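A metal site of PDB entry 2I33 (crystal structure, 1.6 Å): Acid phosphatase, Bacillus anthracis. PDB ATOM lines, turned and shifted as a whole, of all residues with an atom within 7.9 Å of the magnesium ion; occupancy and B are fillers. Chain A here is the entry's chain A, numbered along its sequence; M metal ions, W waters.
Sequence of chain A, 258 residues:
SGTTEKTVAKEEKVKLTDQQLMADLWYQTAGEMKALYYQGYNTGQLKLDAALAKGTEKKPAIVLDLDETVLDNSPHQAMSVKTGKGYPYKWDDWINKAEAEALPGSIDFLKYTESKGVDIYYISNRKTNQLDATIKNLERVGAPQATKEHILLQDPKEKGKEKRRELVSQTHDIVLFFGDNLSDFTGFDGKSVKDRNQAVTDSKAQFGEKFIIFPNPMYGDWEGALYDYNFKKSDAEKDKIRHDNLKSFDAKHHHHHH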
ATOM      1  N   TYR A  27     -21.648  -1.575  -4.517  1.00  0.00           N
ATOM      2  CA  TYR A  27     -20.516  -1.865  -3.656  1.00  0.00           C
ATOM      3  C   TYR A  27     -20.990  -2.547  -2.362  1.00  0.00           C
ATOM      4  O   TYR A  27     -20.340  -3.482  -1.850  1.00  0.00           O
ATOM      5  CB  TYR A  27     -19.801  -0.580  -3.315  1.00  0.00           C
ATOM      6  CG  TYR A  27     -18.467  -0.859  -2.676  1.00  0.00           C
ATOM      7  CD1 TYR A  27     -17.354  -1.084  -3.445  1.00  0.00           C
ATOM      8  CD2 TYR A  27     -18.339  -0.907  -1.298  1.00  0.00           C
ATOM      9  CE1 TYR A  27     -16.094  -1.363  -2.863  1.00  0.00           C
ATOM     10  CE2 TYR A  27     -17.102  -1.205  -0.717  1.00  0.00           C
ATOM     11  CZ  TYR A  27     -15.988  -1.448  -1.486  1.00  0.00           C
ATOM     12  OH  TYR A  27     -14.764  -1.712  -0.915  1.00  0.00           O
ATOM     13  N   TYR A  37     -13.424  -8.963  -4.965  1.00  0.00           N
ATOM     14  CA  TYR A  37     -12.508  -8.944  -3.834  1.00  0.00           C
ATOM     15  C   TYR A  37     -11.877 -10.324  -3.624  1.00  0.00           C
ATOM     16  O   TYR A  37     -10.672 -10.429  -3.485  1.00  0.00           O
ATOM     17  CB  TYR A  37     -13.173  -8.411  -2.568  1.00  0.00           C
ATOM     18  CG  TYR A  37     -13.130  -6.898  -2.567  1.00  0.00           C
ATOM     19  CD1 TYR A  37     -14.101  -6.171  -3.239  1.00  0.00           C
ATOM     20  CD2 TYR A  37     -12.089  -6.201  -1.995  1.00  0.00           C
ATOM     21  CE1 TYR A  37     -14.057  -4.782  -3.299  1.00  0.00           C
ATOM     22  CE2 TYR A  37     -12.039  -4.800  -2.075  1.00  0.00           C
ATOM     23  CZ  TYR A  37     -13.016  -4.102  -2.712  1.00  0.00           C
ATOM     24  OH  TYR A  37     -12.992  -2.736  -2.766  1.00  0.00           O
ATOM     25  N   LEU A  64      -0.647  -2.737   1.127  1.00  0.00           N
ATOM     26  CA  LEU A  64      -2.058  -2.573   0.868  1.00  0.00           C
ATOM     27  C   LEU A  64      -2.548  -1.217   1.270  1.00  0.00           C
ATOM     28  O   LEU A  64      -2.194  -0.667   2.298  1.00  0.00           O
ATOM     29  CB  LEU A  64      -2.877  -3.592   1.633  1.00  0.00           C
ATOM     30  CG  LEU A  64      -2.439  -5.039   1.534  1.00  0.00           C
ATOM     31  CD1 LEU A  64      -1.544  -5.431   2.716  1.00  0.00           C
ATOM     32  CD2 LEU A  64      -3.638  -5.938   1.463  1.00  0.00           C
ATOM     33  N   ASP A  65      -3.440  -0.687   0.446  1.00  0.00           N
ATOM     34  CA  ASP A  65      -4.263   0.411   0.844  1.00  0.00           C
ATOM     35  C   ASP A  65      -5.239  -0.122   1.908  1.00  0.00           C
ATOM     36  O   ASP A  65      -5.427  -1.321   2.028  1.00  0.00           O
ATOM     37  CB  ASP A  65      -5.003   0.873  -0.418  1.00  0.00           C
ATOM     38  CG  ASP A  65      -6.001   1.882  -0.155  1.00  0.00           C
ATOM     39  OD1 ASP A  65      -5.672   2.899   0.490  1.00  0.00           O
ATOM     40  OD2 ASP A  65      -7.169   1.616  -0.587  1.00  0.00           O
ATOM     41  N   LEU A  66      -5.909   0.788   2.638  1.00  0.00           N
ATOM     42  CA  LEU A  66      -6.889   0.363   3.636  1.00  0.00           C
ATOM     43  C   LEU A  66      -8.290   0.537   3.128  1.00  0.00           C
ATOM     44  O   LEU A  66      -8.990  -0.429   2.951  1.00  0.00           O
ATOM     45  CB  LEU A  66      -6.720   1.068   4.970  1.00  0.00           C
ATOM     46  CG  LEU A  66      -5.511   0.573   5.794  1.00  0.00           C
ATOM     47  CD1 LEU A  66      -5.341   1.367   7.019  1.00  0.00           C
ATOM     48  CD2 LEU A  66      -5.689  -0.901   6.163  1.00  0.00           C
ATOM     49  N   ASP A  67      -8.688   1.774   2.888  1.00  0.00           N
ATOM     50  CA  ASP A  67     -10.101   2.054   2.618  1.00  0.00           C
ATOM     51  C   ASP A  67     -10.452   1.533   1.226  1.00  0.00           C
ATOM     52  O   ASP A  67      -9.857   1.895   0.215  1.00  0.00           O
ATOM     53  CB  ASP A  67     -10.392   3.552   2.772  1.00  0.00           C
ATOM     54  CG  ASP A  67     -10.131   4.039   4.185  1.00  0.00           C
ATOM     55  OD1 ASP A  67     -10.581   3.376   5.125  1.00  0.00           O
ATOM     56  OD2 ASP A  67      -9.418   5.069   4.362  1.00  0.00           O
ATOM     57  N   GLU A  68     -11.475   0.698   1.207  1.00  0.00           N
ATOM     58  CA  GLU A  68     -11.938   0.060  -0.015  1.00  0.00           C
ATOM     59  C   GLU A  68     -10.937  -0.970  -0.597  1.00  0.00           C
ATOM     60  O   GLU A  68     -11.082  -1.419  -1.736  1.00  0.00           O
ATOM     61  CB  GLU A  68     -12.407   1.060  -1.044  1.00  0.00           C
ATOM     62  CG  GLU A  68     -13.820   1.606  -0.746  1.00  0.00           C
ATOM     63  CD  GLU A  68     -14.075   2.046   0.675  1.00  0.00           C
ATOM     64  OE1 GLU A  68     -13.661   3.175   1.042  1.00  0.00           O
ATOM     65  OE2 GLU A  68     -14.741   1.272   1.406  1.00  0.00           O
ATOM     66  N   THR A  69      -9.995  -1.387   0.229  1.00  0.00           N
ATOM     67  CA  THR A  69      -9.109  -2.474  -0.100  1.00  0.00           C
ATOM     68  C   THR A  69      -9.163  -3.532   0.988  1.00  0.00           C
ATOM     69  O   THR A  69      -9.422  -4.701   0.702  1.00  0.00           O
ATOM     70  CB  THR A  69      -7.672  -1.957  -0.295  1.00  0.00           C
ATOM     71  OG1 THR A  69      -7.672  -1.054  -1.412  1.00  0.00           O
ATOM     72  CG2 THR A  69      -6.767  -3.092  -0.535  1.00  0.00           C
ATOM     73  N   VAL A  70      -8.970  -3.105   2.246  1.00  0.00           N
ATOM     74  CA  VAL A  70      -9.072  -3.954   3.438  1.00  0.00           C
ATOM     75  C   VAL A  70     -10.338  -3.604   4.224  1.00  0.00           C
ATOM     76  O   VAL A  70     -11.041  -4.481   4.677  1.00  0.00           O
ATOM     77  CB  VAL A  70      -7.846  -3.837   4.355  1.00  0.00           C
ATOM     78  CG1 VAL A  70      -8.028  -4.654   5.594  1.00  0.00           C
ATOM     79  CG2 VAL A  70      -6.575  -4.244   3.591  1.00  0.00           C
ATOM     80  N   LEU A  71     -10.590  -2.316   4.409  1.00  0.00           N
ATOM     81  CA  LEU A  71     -11.729  -1.854   5.212  1.00  0.00           C
ATOM     82  C   LEU A  71     -12.826  -1.256   4.353  1.00  0.00           C
ATOM     83  O   LEU A  71     -12.575  -0.448   3.469  1.00  0.00           O
ATOM     84  CB  LEU A  71     -11.256  -0.795   6.225  1.00  0.00           C
ATOM     85  CG  LEU A  71     -10.249  -1.282   7.286  1.00  0.00           C
ATOM     86  CD1 LEU A  71      -9.761  -0.116   8.156  1.00  0.00           C
ATOM     87  CD2 LEU A  71     -10.786  -2.404   8.130  1.00  0.00           C
ATOM     88  N   ASN A  73     -15.762   1.127   3.884  1.00  0.00           N
ATOM     89  CA  ASN A  73     -16.349   2.387   4.372  1.00  0.00           C
ATOM     90  C   ASN A  73     -17.638   2.725   3.700  1.00  0.00           C
ATOM     91  O   ASN A  73     -18.149   3.862   3.814  1.00  0.00           O
ATOM     92  CB  ASN A  73     -15.360   3.509   4.175  1.00  0.00           C
ATOM     93  CG  ASN A  73     -14.097   3.221   4.829  1.00  0.00           C
ATOM     94  OD1 ASN A  73     -13.997   3.253   6.052  1.00  0.00           O
ATOM     95  ND2 ASN A  73     -13.108   2.895   4.036  1.00  0.00           N
ATOM     96  N   LEU A 103     -12.992  -6.353   4.133  1.00  0.00           N
ATOM     97  CA  LEU A 103     -13.480  -6.694   2.816  1.00  0.00           C
ATOM     98  C   LEU A 103     -13.221  -8.170   2.509  1.00  0.00           C
ATOM     99  O   LEU A 103     -12.321  -8.800   3.087  1.00  0.00           O
ATOM    100  CB  LEU A 103     -12.882  -5.742   1.783  1.00  0.00           C
ATOM    101  CG  LEU A 103     -13.497  -4.342   1.817  1.00  0.00           C
ATOM    102  CD1 LEU A 103     -12.606  -3.238   1.234  1.00  0.00           C
ATOM    103  CD2 LEU A 103     -14.837  -4.354   1.135  1.00  0.00           C
ATOM    104  N   ILE A 123      -0.448   1.092   3.692  1.00  0.00           N
ATOM    105  CA  ILE A 123      -0.153   2.456   3.295  1.00  0.00           C
ATOM    106  C   ILE A 123      -1.485   3.078   2.896  1.00  0.00           C
ATOM    107  O   ILE A 123      -2.036   2.725   1.865  1.00  0.00           O
ATOM    108  CB  ILE A 123       0.875   2.498   2.163  1.00  0.00           C
ATOM    109  CG1 ILE A 123       2.160   1.800   2.623  1.00  0.00           C
ATOM    110  CG2 ILE A 123       1.154   3.948   1.755  1.00  0.00           C
ATOM    111  CD1 ILE A 123       3.239   1.692   1.571  1.00  0.00           C
ATOM    112  N   SER A 124      -1.950   4.013   3.702  1.00  0.00           N
ATOM    113  CA  SER A 124      -3.314   4.551   3.615  1.00  0.00           C
ATOM    114  C   SER A 124      -3.300   6.054   3.755  1.00  0.00           C
ATOM    115  O   SER A 124      -2.486   6.587   4.495  1.00  0.00           O
ATOM    116  CB  SER A 124      -4.128   3.954   4.753  1.00  0.00           C
ATOM    117  OG  SER A 124      -5.315   4.690   4.969  1.00  0.00           O
ATOM    118  N   ASN A 125      -4.182   6.739   3.036  1.00  0.00           N
ATOM    119  CA  ASN A 125      -4.311   8.182   3.164  1.00  0.00           C
ATOM    120  C   ASN A 125      -5.288   8.673   4.238  1.00  0.00           C
ATOM    121  O   ASN A 125      -5.609   9.866   4.298  1.00  0.00           O
ATOM    122  CB  ASN A 125      -4.540   8.832   1.811  1.00  0.00           C
ATOM    123  CG  ASN A 125      -3.321   8.696   0.908  1.00  0.00           C
ATOM    124  OD1 ASN A 125      -2.249   8.357   1.396  1.00  0.00           O
ATOM    125  ND2 ASN A 125      -3.479   8.965  -0.379  1.00  0.00           N
ATOM    126  N   LYS A 161       1.405   8.561  -2.041  1.00  0.00           N
ATOM    127  CA  LYS A 161       1.971   7.509  -1.214  1.00  0.00           C
ATOM    128  C   LYS A 161       3.397   7.112  -1.572  1.00  0.00           C
ATOM    129  O   LYS A 161       3.975   6.251  -0.919  1.00  0.00           O
ATOM    130  CB  LYS A 161       1.098   6.256  -1.336  1.00  0.00           C
ATOM    131  CG  LYS A 161      -0.229   6.403  -0.650  1.00  0.00           C
ATOM    132  CD  LYS A 161      -1.134   5.262  -1.034  1.00  0.00           C
ATOM    133  CE  LYS A 161      -2.408   5.266  -0.197  1.00  0.00           C
ATOM    134  NZ  LYS A 161      -3.221   4.061  -0.421  1.00  0.00           N
ATOM    135  N   PHE A 178      -1.668  -3.853  -3.290  1.00  0.00           N
ATOM    136  CA  PHE A 178      -3.119  -4.043  -3.332  1.00  0.00           C
ATOM    137  C   PHE A 178      -3.812  -2.697  -3.205  1.00  0.00           C
ATOM    138  O   PHE A 178      -3.502  -1.938  -2.285  1.00  0.00           O
ATOM    139  CB  PHE A 178      -3.600  -4.944  -2.175  1.00  0.00           C
ATOM    140  CG  PHE A 178      -3.088  -6.369  -2.282  1.00  0.00           C
ATOM    141  CD1 PHE A 178      -3.899  -7.363  -2.753  1.00  0.00           C
ATOM    142  CD2 PHE A 178      -1.783  -6.665  -1.944  1.00  0.00           C
ATOM    143  CE1 PHE A 178      -3.424  -8.646  -2.860  1.00  0.00           C
ATOM    144  CE2 PHE A 178      -1.291  -7.936  -2.063  1.00  0.00           C
ATOM    145  CZ  PHE A 178      -2.117  -8.930  -2.515  1.00  0.00           C
ATOM    146  N   GLY A 179      -4.780  -2.421  -4.064  1.00  0.00           N
ATOM    147  CA  GLY A 179      -5.514  -1.173  -3.882  1.00  0.00           C
ATOM    148  C   GLY A 179      -6.732  -1.046  -4.776  1.00  0.00           C
ATOM    149  O   GLY A 179      -6.941  -1.855  -5.650  1.00  0.00           O
ATOM    150  N   ASP A 180      -7.500  -0.001  -4.535  1.00  0.00           N
ATOM    151  CA  ASP A 180      -8.705   0.292  -5.318  1.00  0.00           C
ATOM    152  C   ASP A 180      -8.553   1.554  -6.139  1.00  0.00           C
ATOM    153  O   ASP A 180      -9.466   1.941  -6.868  1.00  0.00           O
ATOM    154  CB  ASP A 180      -9.916   0.481  -4.408  1.00  0.00           C
ATOM    155  CG  ASP A 180      -9.751   1.694  -3.493  1.00  0.00           C
ATOM    156  OD1 ASP A 180      -8.873   1.622  -2.604  1.00  0.00           O
ATOM    157  OD2 ASP A 180     -10.511   2.673  -3.697  1.00  0.00           O
ATOM    158  N   ASN A 181      -7.422   2.197  -6.005  1.00  0.00           N
ATOM    159  CA  ASN A 181      -7.170   3.459  -6.624  1.00  0.00           C
ATOM    160  C   ASN A 181      -5.800   3.334  -7.264  1.00  0.00           C
ATOM    161  O   ASN A 181      -4.883   2.793  -6.658  1.00  0.00           O
ATOM    162  CB  ASN A 181      -7.148   4.513  -5.526  1.00  0.00           C
ATOM    163  CG  ASN A 181      -6.979   5.918  -6.057  1.00  0.00           C
ATOM    164  OD1 ASN A 181      -6.325   6.178  -7.103  1.00  0.00           O
ATOM    165  ND2 ASN A 181      -7.535   6.875  -5.310  1.00  0.00           N
ATOM    166  N   ASP A 184      -2.612   3.857  -5.509  1.00  0.00           N
ATOM    167  CA  ASP A 184      -2.128   2.833  -4.570  1.00  0.00           C
ATOM    168  C   ASP A 184      -0.975   2.013  -5.157  1.00  0.00           C
ATOM    169  O   ASP A 184      -0.371   1.196  -4.460  1.00  0.00           O
ATOM    170  CB  ASP A 184      -3.257   1.899  -4.185  1.00  0.00           C
ATOM    171  CG  ASP A 184      -4.404   2.623  -3.510  1.00  0.00           C
ATOM    172  OD1 ASP A 184      -4.193   3.712  -2.928  1.00  0.00           O
ATOM    173  OD2 ASP A 184      -5.535   2.086  -3.583  1.00  0.00           O
ATOM    174  N   ASN A 216     -13.797   0.100  -7.015  1.00  0.00           N
ATOM    175  CA  ASN A 216     -14.401   1.160  -6.211  1.00  0.00           C
ATOM    176  C   ASN A 216     -14.995   2.255  -7.113  1.00  0.00           C
ATOM    177  O   ASN A 216     -14.356   3.248  -7.440  1.00  0.00           O
ATOM    178  CB  ASN A 216     -13.389   1.780  -5.271  1.00  0.00           C
ATOM    179  CG  ASN A 216     -13.992   2.899  -4.440  1.00  0.00           C
ATOM    180  OD1 ASN A 216     -15.215   3.154  -4.570  1.00  0.00           O
ATOM    181  ND2 ASN A 216     -13.184   3.544  -3.619  1.00  0.00           N
ATOM    182  N   TYR A 219     -15.963   6.412  -5.378  1.00  0.00           N
ATOM    183  CA  TYR A 219     -15.105   7.567  -5.198  1.00  0.00           C
ATOM    184  C   TYR A 219     -13.659   7.190  -5.526  1.00  0.00           C
ATOM    185  O   TYR A 219     -13.318   6.013  -5.677  1.00  0.00           O
ATOM    186  CB  TYR A 219     -15.198   8.075  -3.756  1.00  0.00           C
ATOM    187  CG  TYR A 219     -14.458   7.193  -2.789  1.00  0.00           C
ATOM    188  CD1 TYR A 219     -15.111   6.241  -2.046  1.00  0.00           C
ATOM    189  CD2 TYR A 219     -13.085   7.295  -2.653  1.00  0.00           C
ATOM    190  CE1 TYR A 219     -14.446   5.445  -1.166  1.00  0.00           C
ATOM    191  CE2 TYR A 219     -12.384   6.454  -1.783  1.00  0.00           C
ATOM    192  CZ  TYR A 219     -13.065   5.523  -1.050  1.00  0.00           C
ATOM    193  OH  TYR A 219     -12.341   4.718  -0.193  1.00  0.00           O
ATOM    194  N   GLY A 220     -12.826   8.208  -5.601  1.00  0.00           N
ATOM    195  CA  GLY A 220     -11.415   8.006  -5.802  1.00  0.00           C
ATOM    196  C   GLY A 220     -10.814   8.995  -6.757  1.00  0.00           C
ATOM    197  O   GLY A 220     -11.442  10.017  -7.127  1.00  0.00           O
HETATM  198 MG    MG M   1      -8.579   3.076  -1.043  1.00  0.00          MG
HETATM  199  O   HOH W   1      -7.097   3.969  -2.260  1.00  0.00           O
HETATM  200  O   HOH W   2      -8.073   4.576   0.474  1.00  0.00           O
HETATM  201  O   HOH W   3      -9.958   4.158  -1.621  1.00  0.00           O
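The side-chain carboxylate of Asp 65 lies close to the side-chain hydroxyl of Thr 69, at 2.8 Å. OD1 of Asp 67 sits at hydrogen-bond distance from ND2 of Asn 73 (2.8 Å). NZ of Lys 161 is in salt-bridge range of OD1 of Asp 65 (2.9 Å). N of Asp 65 is in hydrogen-bond range of O of Phe 178 (3.0 Å). The side-chain carboxylate (OD2) of Asp 184 is in hydrogen-bond range of the backbone NH (N) of Asp 180. OD2 of Asp 180 is in hydrogen-bond range of ND2 of Asn 216 (2.8 Å). The side-chain hydroxyl (OG1) of Thr 69 sits at hydrogen-bond distance from the backbone NH (N) of Asp 180, at 3.3 Å.
Three residues have an atom within 4 Å of the magnesium ion: Asp 65, Asp 67 and Asp 180.
The magnesium ion is bound by water W3 (1.8 Å), the side-chain carboxylate of Asp 65 (2.1 Å), water W1 (2.1 Å), the backbone carbonyl oxygen of Asp 67 (2.1 Å), the side-chain carboxylate of Asp 180 (2.2 Å) and water W2 (2.2 Å). The magnesium ion has six donor atoms within binding distance.
Water W1 bridges the side-chain carboxylate of Asp 184 (2.8 Å) and the side-chain carboxylate of Asp 65 (3.3 Å). Water W3 lies within hydrogen-bond range of OD2 of Asp 180 and OH of Tyr 219.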
